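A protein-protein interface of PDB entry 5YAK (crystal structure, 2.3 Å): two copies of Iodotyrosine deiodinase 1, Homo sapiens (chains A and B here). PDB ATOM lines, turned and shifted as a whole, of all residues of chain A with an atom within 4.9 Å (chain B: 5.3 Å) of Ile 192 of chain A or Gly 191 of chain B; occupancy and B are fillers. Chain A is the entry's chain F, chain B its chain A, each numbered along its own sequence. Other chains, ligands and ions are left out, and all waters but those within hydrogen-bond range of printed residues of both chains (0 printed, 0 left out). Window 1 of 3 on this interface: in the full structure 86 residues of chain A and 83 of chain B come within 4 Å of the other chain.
Ile 192 of chain A touches just these residues of chain B: Leu 66 (3.7 Å) and Gly 191 (3.7 Å).
Of chain A, only Ile 188 and Ile 192 come within 4 Å of Gly 191 of chain B.
Printed residues of chain B within 4 Å of Thr 91 of chain A: Phe 62 and Leu 66.
Printed residues of chain A within 4 Å of Ser 187 of chain B: Ile 188 (3.4 Å).
Of the printed residues of chain A, Leu 194 of chain B touches Pro 96 (3.7 Å).
Cys 190 of chain B touches none of the printed residues of chain A.
Leu 193 of chain B touches none of the printed residues of chain A.
The nearest residue of chain B that does not touch Ile 192 of chain A is Ile 192 of chain B (4.5 Å).
The nearest printed residue of chain B that does not touch Ala 196 of chain A is Leu 66 of chain B (6.0 Å).
Ile 188 of chain A touches Gly 191 of chain B, and with the chains exchanged Gly 191 of chain A touches Ile 188 of chain B.
Gly 191 of chain A touches Ile 192 of chain B, and with the chains exchanged Ile 192 of chain A touches Gly 191 of chain B.
Leu 194 of chain A touches Ile 188 of chain B, but with the chains exchanged Ile 188 of chain A does not touch Leu 194 of chain B (4.03 Å).
Positions printed for both chains: 188, 189, 190, 191, 192, 193, 194, 195 and 196.
O of Thr 91 of chain A is in hydrogen-bond range of OG1 of Thr 94 of chain A, 2.5 Å away.
Among the printed residues, pairs that only touch across the chains: Ile 188 of chain A with Ser 187 of chain B (3.4 Å), Gly 191 of chain A with Ile 192 of chain B (3.4 Å), Thr 91 of chain A with Leu 66 of chain B (3.5 Å), Ile 188 of chain A with Gly 191 of chain B (3.5 Å), Ala 196 of chain A with Phe 62 of chain B (3.6 Å), Gly 191 of chain A with Ile 188 of chain B (3.7 Å), Ile 192 of chain A with Leu 66 of chain B (3.7 Å), Thr 94 of chain A with Leu 66 of chain B (3.7 Å), Pro 96 of chain A with Leu 194 of chain B (3.7 Å), Ile 192 of chain A with Gly 191 of chain B (3.7 Å), Leu 194 of chain A with Ile 188 of chain B (3.8 Å) and Thr 91 of chain A with Phe 62 of chain B (3.95 Å).
Hydrophobic or aromatic side chains of chain A within 4 Å of the printed part of chain B: Pro 96, Ile 188, Ile 192, Leu 194 and Ala 196.
Of the 13 printed residues of chain B, 7 touch a printed residue of chain A.
Hydrophobic or aromatic side chains of chain B within 4 Å of the printed part of chain A: Phe 62, Leu 66, Ile 188, Ile 192 and Leu 194.
Among the printed residues, 12 pairs touch across the chains.
Among the printed residues, no Asp or Glu carboxylate lies within 4 Å of a Lys or Arg side-chain nitrogen of the other chain.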
ATOM      1  N   THR A  91      11.883 -27.840  -7.059  1.00  0.00           N
ATOM      2  CA  THR A  91      11.024 -27.497  -5.934  1.00  0.00           C
ATOM      3  C   THR A  91       9.811 -28.470  -5.817  1.00  0.00           C
ATOM      4  O   THR A  91       9.526 -28.991  -4.718  1.00  0.00           O
ATOM      5  CB  THR A  91      10.553 -26.044  -6.053  1.00  0.00           C
ATOM      6  OG1 THR A  91      11.701 -25.194  -6.128  1.00  0.00           O
ATOM      7  CG2 THR A  91       9.759 -25.638  -4.857  1.00  0.00           C
ATOM      8  N   ALA A  92       9.213 -28.792  -6.964  1.00  0.00           N
ATOM      9  CA  ALA A  92       8.114 -29.759  -7.037  1.00  0.00           C
ATOM     10  C   ALA A  92       8.536 -31.105  -6.488  1.00  0.00           C
ATOM     11  O   ALA A  92       7.763 -31.735  -5.739  1.00  0.00           O
ATOM     12  CB  ALA A  92       7.611 -29.901  -8.464  1.00  0.00           C
ATOM     13  N   THR A  94      10.546 -31.699  -4.061  1.00  0.00           N
ATOM     14  CA  THR A  94      10.610 -31.697  -2.599  1.00  0.00           C
ATOM     15  C   THR A  94       9.310 -32.118  -1.911  1.00  0.00           C
ATOM     16  O   THR A  94       9.243 -32.128  -0.674  1.00  0.00           O
ATOM     17  CB  THR A  94      10.945 -30.288  -2.042  1.00  0.00           C
ATOM     18  OG1 THR A  94       9.860 -29.365  -2.294  1.00  0.00           O
ATOM     19  CG2 THR A  94      12.252 -29.765  -2.659  1.00  0.00           C
ATOM     20  N   ALA A  95       8.262 -32.342  -2.704  1.00  0.00           N
ATOM     21  CA  ALA A  95       6.964 -32.792  -2.196  1.00  0.00           C
ATOM     22  C   ALA A  95       7.056 -34.014  -1.347  1.00  0.00           C
ATOM     23  O   ALA A  95       7.894 -34.871  -1.592  1.00  0.00           O
ATOM     24  CB  ALA A  95       6.025 -33.102  -3.344  1.00  0.00           C
ATOM     25  N   PRO A  96       6.111 -34.160  -0.395  1.00  0.00           N
ATOM     26  CA  PRO A  96       5.926 -35.445   0.256  1.00  0.00           C
ATOM     27  C   PRO A  96       5.389 -36.495  -0.722  1.00  0.00           C
ATOM     28  O   PRO A  96       4.844 -36.136  -1.756  1.00  0.00           O
ATOM     29  CB  PRO A  96       4.910 -35.135   1.327  1.00  0.00           C
ATOM     30  CG  PRO A  96       4.132 -34.009   0.807  1.00  0.00           C
ATOM     31  CD  PRO A  96       5.102 -33.181   0.027  1.00  0.00           C
ATOM     32  N   ILE A 188      -0.014 -33.213  -5.311  1.00  0.00           N
ATOM     33  CA  ILE A 188       0.515 -32.319  -4.284  1.00  0.00           C
ATOM     34  C   ILE A 188       1.802 -31.611  -4.817  1.00  0.00           C
ATOM     35  O   ILE A 188       2.004 -30.403  -4.601  1.00  0.00           O
ATOM     36  CB  ILE A 188       0.832 -33.076  -3.031  1.00  0.00           C
ATOM     37  CG1 ILE A 188      -0.433 -33.327  -2.225  1.00  0.00           C
ATOM     38  CG2 ILE A 188       1.842 -32.319  -2.188  1.00  0.00           C
ATOM     39  CD1 ILE A 188      -0.197 -34.262  -1.042  1.00  0.00           C
ATOM     40  N   ALA A 189       2.654 -32.363  -5.501  1.00  0.00           N
ATOM     41  CA  ALA A 189       3.838 -31.795  -6.110  1.00  0.00           C
ATOM     42  C   ALA A 189       3.442 -30.776  -7.191  1.00  0.00           C
ATOM     43  O   ALA A 189       4.123 -29.794  -7.359  1.00  0.00           O
ATOM     44  CB  ALA A 189       4.691 -32.879  -6.715  1.00  0.00           C
ATOM     45  N   CYS A 190       2.339 -31.017  -7.905  1.00  0.00           N
ATOM     46  CA  CYS A 190       1.862 -30.072  -8.872  1.00  0.00           C
ATOM     47  C   CYS A 190       1.449 -28.765  -8.173  1.00  0.00           C
ATOM     48  O   CYS A 190       1.695 -27.689  -8.691  1.00  0.00           O
ATOM     49  CB  CYS A 190       0.741 -30.653  -9.761  1.00  0.00           C
ATOM     50  SG  CYS A 190       0.003 -29.445 -10.926  1.00  0.00           S
ATOM     51  N   GLY A 191       0.895 -28.861  -6.961  1.00  0.00           N
ATOM     52  CA  GLY A 191       0.524 -27.674  -6.235  1.00  0.00           C
ATOM     53  C   GLY A 191       1.746 -26.861  -5.828  1.00  0.00           C
ATOM     54  O   GLY A 191       1.751 -25.636  -5.911  1.00  0.00           O
ATOM     55  N   ILE A 192       2.747 -27.539  -5.299  1.00  0.00           N
ATOM     56  CA  ILE A 192       4.019 -26.914  -5.043  1.00  0.00           C
ATOM     57  C   ILE A 192       4.631 -26.282  -6.320  1.00  0.00           C
ATOM     58  O   ILE A 192       5.101 -25.156  -6.260  1.00  0.00           O
ATOM     59  CB  ILE A 192       4.992 -27.894  -4.401  1.00  0.00           C
ATOM     60  CG1 ILE A 192       4.568 -28.201  -2.984  1.00  0.00           C
ATOM     61  CG2 ILE A 192       6.386 -27.294  -4.364  1.00  0.00           C
ATOM     62  CD1 ILE A 192       5.345 -29.375  -2.399  1.00  0.00           C
ATOM     63  N   LEU A 193       4.583 -26.976  -7.456  1.00  0.00           N
ATOM     64  CA  LEU A 193       5.083 -26.431  -8.715  1.00  0.00           C
ATOM     65  C   LEU A 193       4.388 -25.133  -9.071  1.00  0.00           C
ATOM     66  O   LEU A 193       5.030 -24.176  -9.479  1.00  0.00           O
ATOM     67  CB  LEU A 193       4.902 -27.416  -9.858  1.00  0.00           C
ATOM     68  CG  LEU A 193       5.309 -26.927 -11.243  1.00  0.00           C
ATOM     69  CD1 LEU A 193       6.761 -26.438 -11.270  1.00  0.00           C
ATOM     70  CD2 LEU A 193       5.188 -28.038 -12.266  1.00  0.00           C
ATOM     71  N   LEU A 194       3.075 -25.080  -8.881  1.00  0.00           N
ATOM     72  CA  LEU A 194       2.343 -23.871  -9.164  1.00  0.00           C
ATOM     73  C   LEU A 194       2.767 -22.693  -8.264  1.00  0.00           C
ATOM     74  O   LEU A 194       2.889 -21.543  -8.710  1.00  0.00           O
ATOM     75  CB  LEU A 194       0.866 -24.133  -9.003  1.00  0.00           C
ATOM     76  CG  LEU A 194       0.252 -25.041 -10.038  1.00  0.00           C
ATOM     77  CD1 LEU A 194      -1.055 -25.583  -9.493  1.00  0.00           C
ATOM     78  CD2 LEU A 194       0.010 -24.296 -11.356  1.00  0.00           C
ATOM     79  N   ALA A 195       2.920 -22.977  -6.980  1.00  0.00           N
ATOM     80  CA  ALA A 195       3.397 -21.981  -6.063  1.00  0.00           C
ATOM     81  C   ALA A 195       4.753 -21.439  -6.561  1.00  0.00           C
ATOM     82  O   ALA A 195       4.948 -20.238  -6.665  1.00  0.00           O
ATOM     83  CB  ALA A 195       3.555 -22.562  -4.675  1.00  0.00           C
ATOM     84  N   ALA A 196       5.668 -22.352  -6.845  1.00  0.00           N
ATOM     85  CA  ALA A 196       6.989 -22.007  -7.282  1.00  0.00           C
ATOM     86  C   ALA A 196       6.958 -21.155  -8.565  1.00  0.00           C
ATOM     87  O   ALA A 196       7.713 -20.224  -8.678  1.00  0.00           O
ATOM     88  CB  ALA A 196       7.818 -23.261  -7.485  1.00  0.00           C
ATOM     89  N   PHE B  62      13.439 -20.181  -3.098  1.00  0.00           N
ATOM     90  CA  PHE B  62      12.192 -20.853  -2.786  1.00  0.00           C
ATOM     91  C   PHE B  62      12.450 -22.355  -2.791  1.00  0.00           C
ATOM     92  O   PHE B  62      12.052 -23.021  -1.848  1.00  0.00           O
ATOM     93  CB  PHE B  62      11.109 -20.482  -3.771  1.00  0.00           C
ATOM     94  CG  PHE B  62       9.741 -20.937  -3.369  1.00  0.00           C
ATOM     95  CD1 PHE B  62       9.017 -21.816  -4.172  1.00  0.00           C
ATOM     96  CD2 PHE B  62       9.169 -20.479  -2.200  1.00  0.00           C
ATOM     97  CE1 PHE B  62       7.745 -22.207  -3.803  1.00  0.00           C
ATOM     98  CE2 PHE B  62       7.890 -20.869  -1.826  1.00  0.00           C
ATOM     99  CZ  PHE B  62       7.180 -21.725  -2.630  1.00  0.00           C
ATOM    100  N   LEU B  66      11.906 -24.816   0.511  1.00  0.00           N
ATOM    101  CA  LEU B  66      11.017 -25.989   0.460  1.00  0.00           C
ATOM    102  C   LEU B  66      11.751 -27.286   0.634  1.00  0.00           C
ATOM    103  O   LEU B  66      11.226 -28.215   1.263  1.00  0.00           O
ATOM    104  CB  LEU B  66      10.165 -26.000  -0.797  1.00  0.00           C
ATOM    105  CG  LEU B  66       9.063 -24.965  -0.736  1.00  0.00           C
ATOM    106  CD1 LEU B  66       8.054 -25.217  -1.827  1.00  0.00           C
ATOM    107  CD2 LEU B  66       8.370 -24.980   0.599  1.00  0.00           C
ATOM    108  N   VAL B 186      -8.226 -30.757  -4.820  1.00  0.00           N
ATOM    109  CA  VAL B 186      -8.002 -30.648  -3.397  1.00  0.00           C
ATOM    110  C   VAL B 186      -6.576 -30.938  -3.032  1.00  0.00           C
ATOM    111  O   VAL B 186      -6.001 -30.268  -2.194  1.00  0.00           O
ATOM    112  CB  VAL B 186      -9.000 -31.461  -2.574  1.00  0.00           C
ATOM    113  CG1 VAL B 186      -8.775 -31.192  -1.102  1.00  0.00           C
ATOM    114  CG2 VAL B 186     -10.425 -31.050  -2.936  1.00  0.00           C
ATOM    115  N   SER B 187      -6.001 -31.915  -3.705  1.00  0.00           N
ATOM    116  CA  SER B 187      -4.649 -32.321  -3.481  1.00  0.00           C
ATOM    117  C   SER B 187      -3.682 -31.218  -3.877  1.00  0.00           C
ATOM    118  O   SER B 187      -2.683 -31.055  -3.242  1.00  0.00           O
ATOM    119  CB  SER B 187      -4.337 -33.545  -4.337  1.00  0.00           C
ATOM    120  OG  SER B 187      -5.072 -34.688  -3.915  1.00  0.00           O
ATOM    121  N   ILE B 188      -4.004 -30.477  -4.935  1.00  0.00           N
ATOM    122  CA  ILE B 188      -3.213 -29.345  -5.368  1.00  0.00           C
ATOM    123  C   ILE B 188      -3.281 -28.259  -4.272  1.00  0.00           C
ATOM    124  O   ILE B 188      -2.256 -27.709  -3.857  1.00  0.00           O
ATOM    125  CB  ILE B 188      -3.729 -28.803  -6.713  1.00  0.00           C
ATOM    126  CG1 ILE B 188      -3.233 -29.663  -7.841  1.00  0.00           C
ATOM    127  CG2 ILE B 188      -3.238 -27.399  -6.920  1.00  0.00           C
ATOM    128  CD1 ILE B 188      -3.910 -29.422  -9.171  1.00  0.00           C
ATOM    129  N   ALA B 189      -4.468 -28.038  -3.727  1.00  0.00           N
ATOM    130  CA  ALA B 189      -4.589 -27.168  -2.580  1.00  0.00           C
ATOM    131  C   ALA B 189      -3.760 -27.577  -1.374  1.00  0.00           C
ATOM    132  O   ALA B 189      -3.243 -26.707  -0.652  1.00  0.00           O
ATOM    133  CB  ALA B 189      -6.040 -26.941  -2.198  1.00  0.00           C
ATOM    134  N   CYS B 190      -3.657 -28.872  -1.119  1.00  0.00           N
ATOM    135  CA  CYS B 190      -2.872 -29.338   0.001  1.00  0.00           C
ATOM    136  C   CYS B 190      -1.384 -29.098  -0.239  1.00  0.00           C
ATOM    137  O   CYS B 190      -0.633 -28.849   0.701  1.00  0.00           O
ATOM    138  CB  CYS B 190      -3.131 -30.853   0.204  1.00  0.00           C
ATOM    139  SG  CYS B 190      -2.176 -31.679   1.513  1.00  0.00           S
ATOM    140  N   GLY B 191      -0.935 -29.227  -1.477  1.00  0.00           N
ATOM    141  CA  GLY B 191       0.465 -28.882  -1.836  1.00  0.00           C
ATOM    142  C   GLY B 191       0.777 -27.421  -1.525  1.00  0.00           C
ATOM    143  O   GLY B 191       1.721 -27.095  -0.841  1.00  0.00           O
ATOM    144  N   ILE B 192      -0.098 -26.542  -1.959  1.00  0.00           N
ATOM    145  CA  ILE B 192       0.052 -25.128  -1.667  1.00  0.00           C
ATOM    146  C   ILE B 192       0.048 -24.866  -0.156  1.00  0.00           C
ATOM    147  O   ILE B 192       0.888 -24.111   0.348  1.00  0.00           O
ATOM    148  CB  ILE B 192      -1.011 -24.336  -2.395  1.00  0.00           C
ATOM    149  CG1 ILE B 192      -0.720 -24.400  -3.909  1.00  0.00           C
ATOM    150  CG2 ILE B 192      -1.067 -22.926  -1.867  1.00  0.00           C
ATOM    151  CD1 ILE B 192      -1.783 -23.743  -4.770  1.00  0.00           C
ATOM    152  N   LEU B 193      -0.862 -25.520   0.565  1.00  0.00           N
ATOM    153  CA  LEU B 193      -0.886 -25.448   2.009  1.00  0.00           C
ATOM    154  C   LEU B 193       0.436 -25.887   2.642  1.00  0.00           C
ATOM    155  O   LEU B 193       0.920 -25.276   3.570  1.00  0.00           O
ATOM    156  CB  LEU B 193      -2.024 -26.295   2.569  1.00  0.00           C
ATOM    157  CG  LEU B 193      -2.192 -26.357   4.091  1.00  0.00           C
ATOM    158  CD1 LEU B 193      -2.357 -24.988   4.720  1.00  0.00           C
ATOM    159  CD2 LEU B 193      -3.408 -27.215   4.405  1.00  0.00           C
ATOM    160  N   LEU B 194       1.010 -26.969   2.171  1.00  0.00           N
ATOM    161  CA  LEU B 194       2.290 -27.403   2.699  1.00  0.00           C
ATOM    162  C   LEU B 194       3.424 -26.376   2.457  1.00  0.00           C
ATOM    163  O   LEU B 194       4.290 -26.189   3.296  1.00  0.00           O
ATOM    164  CB  LEU B 194       2.657 -28.760   2.080  1.00  0.00           C
ATOM    165  CG  LEU B 194       1.768 -29.925   2.544  1.00  0.00           C
ATOM    166  CD1 LEU B 194       1.919 -31.147   1.671  1.00  0.00           C
ATOM    167  CD2 LEU B 194       2.136 -30.329   3.948  1.00  0.00           C
ATOM    168  N   ALA B 195       3.462 -25.757   1.292  1.00  0.00           N
ATOM    169  CA  ALA B 195       4.503 -24.755   1.043  1.00  0.00           C
ATOM    170  C   ALA B 195       4.271 -23.572   1.990  1.00  0.00           C
ATOM    171  O   ALA B 195       5.197 -23.013   2.548  1.00  0.00           O
ATOM    172  CB  ALA B 195       4.446 -24.306  -0.403  1.00  0.00           C
ATOM    173  N   ALA B 196       3.010 -23.212   2.164  1.00  0.00           N
ATOM    174  CA  ALA B 196       2.636 -22.114   3.016  1.00  0.00           C
ATOM    175  C   ALA B 196       3.037 -22.383   4.464  1.00  0.00           C
ATOM    176  O   ALA B 196       3.483 -21.469   5.167  1.00  0.00           O
ATOM    177  CB  ALA B 196       1.142 -21.876   2.921  1.00  0.00           C
